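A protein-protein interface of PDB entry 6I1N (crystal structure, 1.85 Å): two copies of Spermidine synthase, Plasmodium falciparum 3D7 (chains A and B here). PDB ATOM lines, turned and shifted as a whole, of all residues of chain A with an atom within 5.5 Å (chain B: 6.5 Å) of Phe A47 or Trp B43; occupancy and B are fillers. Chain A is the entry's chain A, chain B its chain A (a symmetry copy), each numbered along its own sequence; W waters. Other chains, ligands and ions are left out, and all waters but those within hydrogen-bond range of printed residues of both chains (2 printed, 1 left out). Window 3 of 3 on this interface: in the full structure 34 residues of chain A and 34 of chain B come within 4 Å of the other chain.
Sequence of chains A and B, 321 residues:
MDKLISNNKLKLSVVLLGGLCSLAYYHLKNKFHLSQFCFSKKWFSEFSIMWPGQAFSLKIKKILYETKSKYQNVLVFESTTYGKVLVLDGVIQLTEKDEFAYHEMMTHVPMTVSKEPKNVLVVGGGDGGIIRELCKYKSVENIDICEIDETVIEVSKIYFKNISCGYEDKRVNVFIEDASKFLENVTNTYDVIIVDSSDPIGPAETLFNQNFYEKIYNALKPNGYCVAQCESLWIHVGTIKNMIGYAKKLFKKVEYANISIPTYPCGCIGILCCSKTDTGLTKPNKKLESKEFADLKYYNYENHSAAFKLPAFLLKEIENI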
ATOM      1  N   SER A  45     -13.450   3.773   7.451  1.00  0.00           N
ATOM      2  CA  SER A  45     -14.828   3.923   7.906  1.00  0.00           C
ATOM      3  C   SER A  45     -15.710   2.899   7.210  1.00  0.00           C
ATOM      4  O   SER A  45     -15.617   2.714   5.994  1.00  0.00           O
ATOM      5  CB  SER A  45     -15.365   5.353   7.660  1.00  0.00           C
ATOM      6  OG  SER A  45     -14.732   6.301   8.517  1.00  0.00           O
ATOM      7  N   GLU A  46     -16.549   2.232   7.991  1.00  0.00           N
ATOM      8  CA  GLU A  46     -17.368   1.112   7.540  1.00  0.00           C
ATOM      9  C   GLU A  46     -18.797   1.611   7.332  1.00  0.00           C
ATOM     10  O   GLU A  46     -19.564   1.746   8.292  1.00  0.00           O
ATOM     11  CB  GLU A  46     -17.315  -0.016   8.569  1.00  0.00           C
ATOM     12  CG  GLU A  46     -18.114  -1.230   8.175  1.00  0.00           C
ATOM     13  CD  GLU A  46     -18.161  -2.261   9.259  1.00  0.00           C
ATOM     14  OE1 GLU A  46     -18.532  -1.900  10.396  1.00  0.00           O
ATOM     15  OE2 GLU A  46     -17.848  -3.436   8.984  1.00  0.00           O
ATOM     16  N   PHE A  47     -19.156   1.867   6.080  1.00  0.00           N
ATOM     17  CA  PHE A  47     -20.507   2.228   5.682  1.00  0.00           C
ATOM     18  C   PHE A  47     -21.181   1.054   4.992  1.00  0.00           C
ATOM     19  O   PHE A  47     -20.510   0.195   4.419  1.00  0.00           O
ATOM     20  CB  PHE A  47     -20.508   3.427   4.729  1.00  0.00           C
ATOM     21  CG  PHE A  47     -19.920   4.672   5.314  1.00  0.00           C
ATOM     22  CD1 PHE A  47     -20.696   5.532   6.065  1.00  0.00           C
ATOM     23  CD2 PHE A  47     -18.588   4.987   5.100  1.00  0.00           C
ATOM     24  CE1 PHE A  47     -20.156   6.685   6.607  1.00  0.00           C
ATOM     25  CE2 PHE A  47     -18.042   6.139   5.634  1.00  0.00           C
ATOM     26  CZ  PHE A  47     -18.820   6.988   6.389  1.00  0.00           C
ATOM     27  N   SER A  48     -22.513   1.026   5.031  1.00  0.00           N
ATOM     28  CA  SER A  48     -23.227  -0.029   4.325  1.00  0.00           C
ATOM     29  C   SER A  48     -24.714   0.276   4.322  1.00  0.00           C
ATOM     30  O   SER A  48     -25.248   0.792   5.308  1.00  0.00           O
ATOM     31  CB  SER A  48     -22.975  -1.402   4.967  1.00  0.00           C
ATOM     32  OG  SER A  48     -23.790  -2.404   4.392  1.00  0.00           O
ATOM     33  N   ILE A  49     -25.383  -0.066   3.218  1.00  0.00           N
ATOM     34  CA  ILE A  49     -26.841   0.007   3.174  1.00  0.00           C
ATOM     35  C   ILE A  49     -27.473  -0.970   4.161  1.00  0.00           C
ATOM     36  O   ILE A  49     -28.645  -0.813   4.539  1.00  0.00           O
ATOM     37  CB  ILE A  49     -27.331  -0.242   1.731  1.00  0.00           C
ATOM     38  CG1 ILE A  49     -26.849  -1.604   1.232  1.00  0.00           C
ATOM     39  CG2 ILE A  49     -26.800   0.842   0.799  1.00  0.00           C
ATOM     40  CD1 ILE A  49     -27.813  -2.304   0.314  1.00  0.00           C
ATOM     41  N   TRP A  51     -26.648  -1.298   7.279  1.00  0.00           N
ATOM     42  CA  TRP A  51     -26.846  -0.551   8.523  1.00  0.00           C
ATOM     43  C   TRP A  51     -26.821   0.932   8.181  1.00  0.00           C
ATOM     44  O   TRP A  51     -25.848   1.641   8.479  1.00  0.00           O
ATOM     45  CB  TRP A  51     -25.805  -0.904   9.588  1.00  0.00           C
ATOM     46  CG  TRP A  51     -24.401  -1.128   9.096  1.00  0.00           C
ATOM     47  CD1 TRP A  51     -23.379  -0.209   9.052  1.00  0.00           C
ATOM     48  CD2 TRP A  51     -23.847  -2.360   8.621  1.00  0.00           C
ATOM     49  NE1 TRP A  51     -22.232  -0.795   8.565  1.00  0.00           N
ATOM     50  CE2 TRP A  51     -22.492  -2.117   8.302  1.00  0.00           C
ATOM     51  CE3 TRP A  51     -24.367  -3.644   8.430  1.00  0.00           C
ATOM     52  CZ2 TRP A  51     -21.656  -3.109   7.793  1.00  0.00           C
ATOM     53  CZ3 TRP A  51     -23.534  -4.629   7.922  1.00  0.00           C
ATOM     54  CH2 TRP A  51     -22.196  -4.359   7.614  1.00  0.00           C
ATOM     55  N   PRO A  52     -27.877   1.431   7.543  1.00  0.00           N
ATOM     56  CA  PRO A  52     -27.900   2.840   7.145  1.00  0.00           C
ATOM     57  C   PRO A  52     -27.941   3.767   8.350  1.00  0.00           C
ATOM     58  O   PRO A  52     -28.542   3.471   9.387  1.00  0.00           O
ATOM     59  CB  PRO A  52     -29.194   2.955   6.325  1.00  0.00           C
ATOM     60  CG  PRO A  52     -30.068   1.916   6.858  1.00  0.00           C
ATOM     61  CD  PRO A  52     -29.185   0.779   7.339  1.00  0.00           C
ATOM     62  N   GLY A  53     -27.303   4.913   8.192  1.00  0.00           N
ATOM     63  CA  GLY A  53     -27.368   5.917   9.218  1.00  0.00           C
ATOM     64  C   GLY A  53     -26.343   5.768  10.306  1.00  0.00           C
ATOM     65  O   GLY A  53     -26.351   6.571  11.245  1.00  0.00           O
ATOM     66  N   GLN A  54     -25.482   4.752  10.235  1.00  0.00           N
ATOM     67  CA  GLN A  54     -24.443   4.567  11.237  1.00  0.00           C
ATOM     68  C   GLN A  54     -23.164   4.137  10.547  1.00  0.00           C
ATOM     69  O   GLN A  54     -23.182   3.659   9.414  1.00  0.00           O
ATOM     70  CB  GLN A  54     -24.849   3.518  12.297  1.00  0.00           C
ATOM     71  CG  GLN A  54     -24.882   2.113  11.738  1.00  0.00           C
ATOM     72  CD  GLN A  54     -25.453   1.112  12.719  1.00  0.00           C
ATOM     73  OE1 GLN A  54     -26.671   0.994  12.872  1.00  0.00           O
ATOM     74  NE2 GLN A  54     -24.570   0.394  13.411  1.00  0.00           N
ATOM     75  N   ALA A  55     -22.043   4.300  11.249  1.00  0.00           N
ATOM     76  CA  ALA A  55     -20.761   3.852  10.739  1.00  0.00           C
ATOM     77  C   ALA A  55     -19.797   3.699  11.904  1.00  0.00           C
ATOM     78  O   ALA A  55     -19.870   4.440  12.884  1.00  0.00           O
ATOM     79  CB  ALA A  55     -20.185   4.829   9.693  1.00  0.00           C
ATOM     80  N   GLY A  90     -15.232  -3.415   1.908  1.00  0.00           N
ATOM     81  CA  GLY A  90     -15.439  -2.303   2.818  1.00  0.00           C
ATOM     82  C   GLY A  90     -16.131  -2.647   4.123  1.00  0.00           C
ATOM     83  O   GLY A  90     -16.455  -1.738   4.889  1.00  0.00           O
ATOM     84  N   VAL A  91     -16.355  -3.927   4.401  1.00  0.00           N
ATOM     85  CA  VAL A  91     -16.973  -4.402   5.636  1.00  0.00           C
ATOM     86  C   VAL A  91     -15.917  -5.149   6.441  1.00  0.00           C
ATOM     87  O   VAL A  91     -15.193  -5.990   5.889  1.00  0.00           O
ATOM     88  CB  VAL A  91     -18.177  -5.309   5.335  1.00  0.00           C
ATOM     89  CG1 VAL A  91     -18.603  -6.123   6.588  1.00  0.00           C
ATOM     90  CG2 VAL A  91     -19.341  -4.469   4.797  1.00  0.00           C
ATOM     91  N   LYS B  41     -26.605  15.024   3.714  1.00  0.00           N
ATOM     92  CA  LYS B  41     -26.692  15.294   5.153  1.00  0.00           C
ATOM     93  C   LYS B  41     -25.333  15.073   5.822  1.00  0.00           C
ATOM     94  O   LYS B  41     -24.518  14.309   5.324  1.00  0.00           O
ATOM     95  CB  LYS B  41     -27.759  14.410   5.814  1.00  0.00           C
ATOM     96  CG  LYS B  41     -29.062  14.296   5.036  1.00  0.00           C
ATOM     97  CD  LYS B  41     -30.139  13.599   5.850  1.00  0.00           C
ATOM     98  CE  LYS B  41     -31.342  13.259   4.988  1.00  0.00           C
ATOM     99  NZ  LYS B  41     -32.467  12.719   5.803  1.00  0.00           N
ATOM    100  N   LYS B  42     -25.090  15.744   6.943  1.00  0.00           N
ATOM    101  CA  LYS B  42     -23.846  15.584   7.680  1.00  0.00           C
ATOM    102  C   LYS B  42     -23.954  14.419   8.681  1.00  0.00           C
ATOM    103  O   LYS B  42     -25.012  13.810   8.862  1.00  0.00           O
ATOM    104  CB  LYS B  42     -23.485  16.883   8.399  1.00  0.00           C
ATOM    105  CG  LYS B  42     -22.123  16.881   9.088  1.00  0.00           C
ATOM    106  CD  LYS B  42     -21.064  16.098   8.298  1.00  0.00           C
ATOM    107  CE  LYS B  42     -19.686  16.348   8.884  1.00  0.00           C
ATOM    108  NZ  LYS B  42     -19.435  17.823   8.960  1.00  0.00           N
ATOM    109  N   TRP B  43     -22.830  14.130   9.337  1.00  0.00           N
ATOM    110  CA  TRP B  43     -22.658  13.008  10.249  1.00  0.00           C
ATOM    111  C   TRP B  43     -22.078  13.528  11.552  1.00  0.00           C
ATOM    112  O   TRP B  43     -21.115  14.304  11.539  1.00  0.00           O
ATOM    113  CB  TRP B  43     -21.705  11.941   9.656  1.00  0.00           C
ATOM    114  CG  TRP B  43     -22.307  11.091   8.547  1.00  0.00           C
ATOM    115  CD1 TRP B  43     -22.555  11.477   7.253  1.00  0.00           C
ATOM    116  CD2 TRP B  43     -22.740   9.720   8.638  1.00  0.00           C
ATOM    117  NE1 TRP B  43     -23.121  10.442   6.545  1.00  0.00           N
ATOM    118  CE2 TRP B  43     -23.233   9.349   7.365  1.00  0.00           C
ATOM    119  CE3 TRP B  43     -22.757   8.771   9.669  1.00  0.00           C
ATOM    120  CZ2 TRP B  43     -23.737   8.077   7.101  1.00  0.00           C
ATOM    121  CZ3 TRP B  43     -23.260   7.508   9.399  1.00  0.00           C
ATOM    122  CH2 TRP B  43     -23.749   7.177   8.135  1.00  0.00           C
ATOM    123  N   PHE B  44     -22.652  13.095  12.672  1.00  0.00           N
ATOM    124  CA  PHE B  44     -22.008  13.283  13.961  1.00  0.00           C
ATOM    125  C   PHE B  44     -21.004  12.162  14.176  1.00  0.00           C
ATOM    126  O   PHE B  44     -21.312  11.000  13.924  1.00  0.00           O
ATOM    127  CB  PHE B  44     -23.056  13.279  15.095  1.00  0.00           C
ATOM    128  CG  PHE B  44     -22.446  13.187  16.444  1.00  0.00           C
ATOM    129  CD1 PHE B  44     -21.928  14.312  17.048  1.00  0.00           C
ATOM    130  CD2 PHE B  44     -22.307  11.941  17.086  1.00  0.00           C
ATOM    131  CE1 PHE B  44     -21.302  14.222  18.271  1.00  0.00           C
ATOM    132  CE2 PHE B  44     -21.694  11.855  18.306  1.00  0.00           C
ATOM    133  CZ  PHE B  44     -21.201  13.001  18.913  1.00  0.00           C
ATOM    134  N   SER B  45     -19.827  12.492  14.707  1.00  0.00           N
ATOM    135  CA  SER B  45     -18.815  11.476  14.971  1.00  0.00           C
ATOM    136  C   SER B  45     -18.301  11.625  16.395  1.00  0.00           C
ATOM    137  O   SER B  45     -18.004  12.736  16.840  1.00  0.00           O
ATOM    138  CB  SER B  45     -17.642  11.553  13.965  1.00  0.00           C
ATOM    139  OG  SER B  45     -18.048  11.143  12.660  1.00  0.00           O
ATOM    140  N   SER B  57     -20.328   6.844  14.452  1.00  0.00           N
ATOM    141  CA  SER B  57     -20.962   7.982  13.793  1.00  0.00           C
ATOM    142  C   SER B  57     -22.414   7.694  13.476  1.00  0.00           C
ATOM    143  O   SER B  57     -22.771   6.570  13.123  1.00  0.00           O
ATOM    144  CB  SER B  57     -20.257   8.359  12.465  1.00  0.00           C
ATOM    145  OG  SER B  57     -18.902   8.675  12.694  1.00  0.00           O
ATOM    146  N   LEU B  58     -23.243   8.734  13.565  1.00  0.00           N
ATOM    147  CA  LEU B  58     -24.655   8.660  13.233  1.00  0.00           C
ATOM    148  C   LEU B  58     -24.956   9.722  12.199  1.00  0.00           C
ATOM    149  O   LEU B  58     -24.396  10.821  12.256  1.00  0.00           O
ATOM    150  CB  LEU B  58     -25.530   8.901  14.443  1.00  0.00           C
ATOM    151  CG  LEU B  58     -25.491   7.756  15.450  1.00  0.00           C
ATOM    152  CD1 LEU B  58     -26.252   8.223  16.673  1.00  0.00           C
ATOM    153  CD2 LEU B  58     -26.127   6.527  14.840  1.00  0.00           C
ATOM    154  N   LYS B  59     -25.848   9.404  11.270  1.00  0.00           N
ATOM    155  CA  LYS B  59     -26.243  10.383  10.272  1.00  0.00           C
ATOM    156  C   LYS B  59     -27.283  11.327  10.872  1.00  0.00           C
ATOM    157  O   LYS B  59     -28.222  10.886  11.555  1.00  0.00           O
ATOM    158  CB  LYS B  59     -26.789   9.692   9.024  1.00  0.00           C
ATOM    159  CG  LYS B  59     -26.744  10.548   7.737  1.00  0.00           C
ATOM    160  CD  LYS B  59     -27.401   9.781   6.574  1.00  0.00           C
ATOM    161  CE  LYS B  59     -27.333  10.541   5.263  1.00  0.00           C
ATOM    162  NZ  LYS B  59     -27.954   9.756   4.149  1.00  0.00           N
ATOM    163  N   ILE B  60     -27.118  12.625  10.604  1.00  0.00           N
ATOM    164  CA  ILE B  60     -27.972  13.665  11.181  1.00  0.00           C
ATOM    165  C   ILE B  60     -29.117  13.958  10.225  1.00  0.00           C
ATOM    166  O   ILE B  60     -28.885  14.391   9.097  1.00  0.00           O
ATOM    167  CB  ILE B  60     -27.182  14.949  11.459  1.00  0.00           C
ATOM    168  CG1 ILE B  60     -26.025  14.670  12.413  1.00  0.00           C
ATOM    169  CG2 ILE B  60     -28.143  16.042  12.007  1.00  0.00           C
ATOM    170  CD1 ILE B  60     -24.866  15.648  12.313  1.00  0.00           C
ATOM    171  N   THR B  80     -30.967   9.898  11.522  1.00  0.00           N
ATOM    172  CA  THR B  80     -31.817   9.247  10.524  1.00  0.00           C
ATOM    173  C   THR B  80     -32.327   7.880  10.976  1.00  0.00           C
ATOM    174  O   THR B  80     -33.426   7.472  10.583  1.00  0.00           O
ATOM    175  CB  THR B  80     -31.075   9.116   9.194  1.00  0.00           C
ATOM    176  OG1 THR B  80     -29.944   8.257   9.348  1.00  0.00           O
ATOM    177  CG2 THR B  80     -30.599  10.478   8.732  1.00  0.00           C
HETATM  178  O   HOH W   1     -28.950   7.573  12.362  1.00  0.00           O
HETATM  179  O   HOH W   2     -17.356   6.431  12.493  1.00  0.00           O
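Of the printed residues of chain B, Phe A47 touches Trp B43 (3.9 Å). Printed residues of chain A within 4 Å of Ser B57: Gln A54 and Ala A55. Of the printed residues of chain A, Thr B80 touches Gly A53 (3.5 Å). Of the printed residues of chain B, Gly A53 touches Trp B43, Leu B58, Lys B59 and Thr B80. Printed residues of chain B within 4 Å of Ala A55: Trp B43 (3.9 Å) and Ser B57 (2.9 Å). Lys B42 touches none of the printed residues of chain A. The nearest residue of chain B that does not touch Phe A47 is Ser B57 (6.1 Å). The nearest printed residue of chain A that does not touch Ser B57 is Gly A53 (4.04 Å).
Among the printed residues, pairs that only touch across the chains: Gln A54 with Ser B57 (3.2 Å), Gly A53 with Leu B58 (3.3 Å), Gly A53 with Thr B80 (3.5 Å), Gln A54 with Trp B43 (3.6 Å), Gly A53 with Trp B43 (3.7 Å), Phe A47 with Trp B43 (3.9 Å) and Ala A55 with Trp B43 (3.9 Å).
OG of Ser B45 is in hydrogen-bond range of OG of Ser B57 (2.6 Å). The backbone carbonyl oxygen of Lys B59 is in hydrogen-bond range of the backbone NH of Thr B80. The backbone carbonyl oxygen of Leu B58 lies within hydrogen-bond range of the backbone NH of Phe B44 (2.9 Å).
Of the 10 printed residues of chain B, 5 touch a printed residue of chain A. Among the printed residues, 9 pairs touch across the chains.
The backbone NH of Lys B59 lies within hydrogen-bond range of the backbone carbonyl oxygen of Gly A53, at 2.9 Å. The backbone NH (N) of Ser B57 is in hydrogen-bond range of the backbone carbonyl oxygen (O) of Ala A55 (2.9 Å).
1 position is printed for both chains. Of the 9 pairs that touch across the chains among the printed residues, none has its exchanged pair printed and touching as well.
Water W2 bridges OG of Ser B57 and O of Ala A55. Water W1 lies within hydrogen-bond range of the backbone carbonyl oxygen (O) of Gly A53 (3.0 Å), the backbone NH (N) of Thr B80 (3.2 Å) and the backbone carbonyl oxygen (O) of Lys B59 (3.5 Å).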
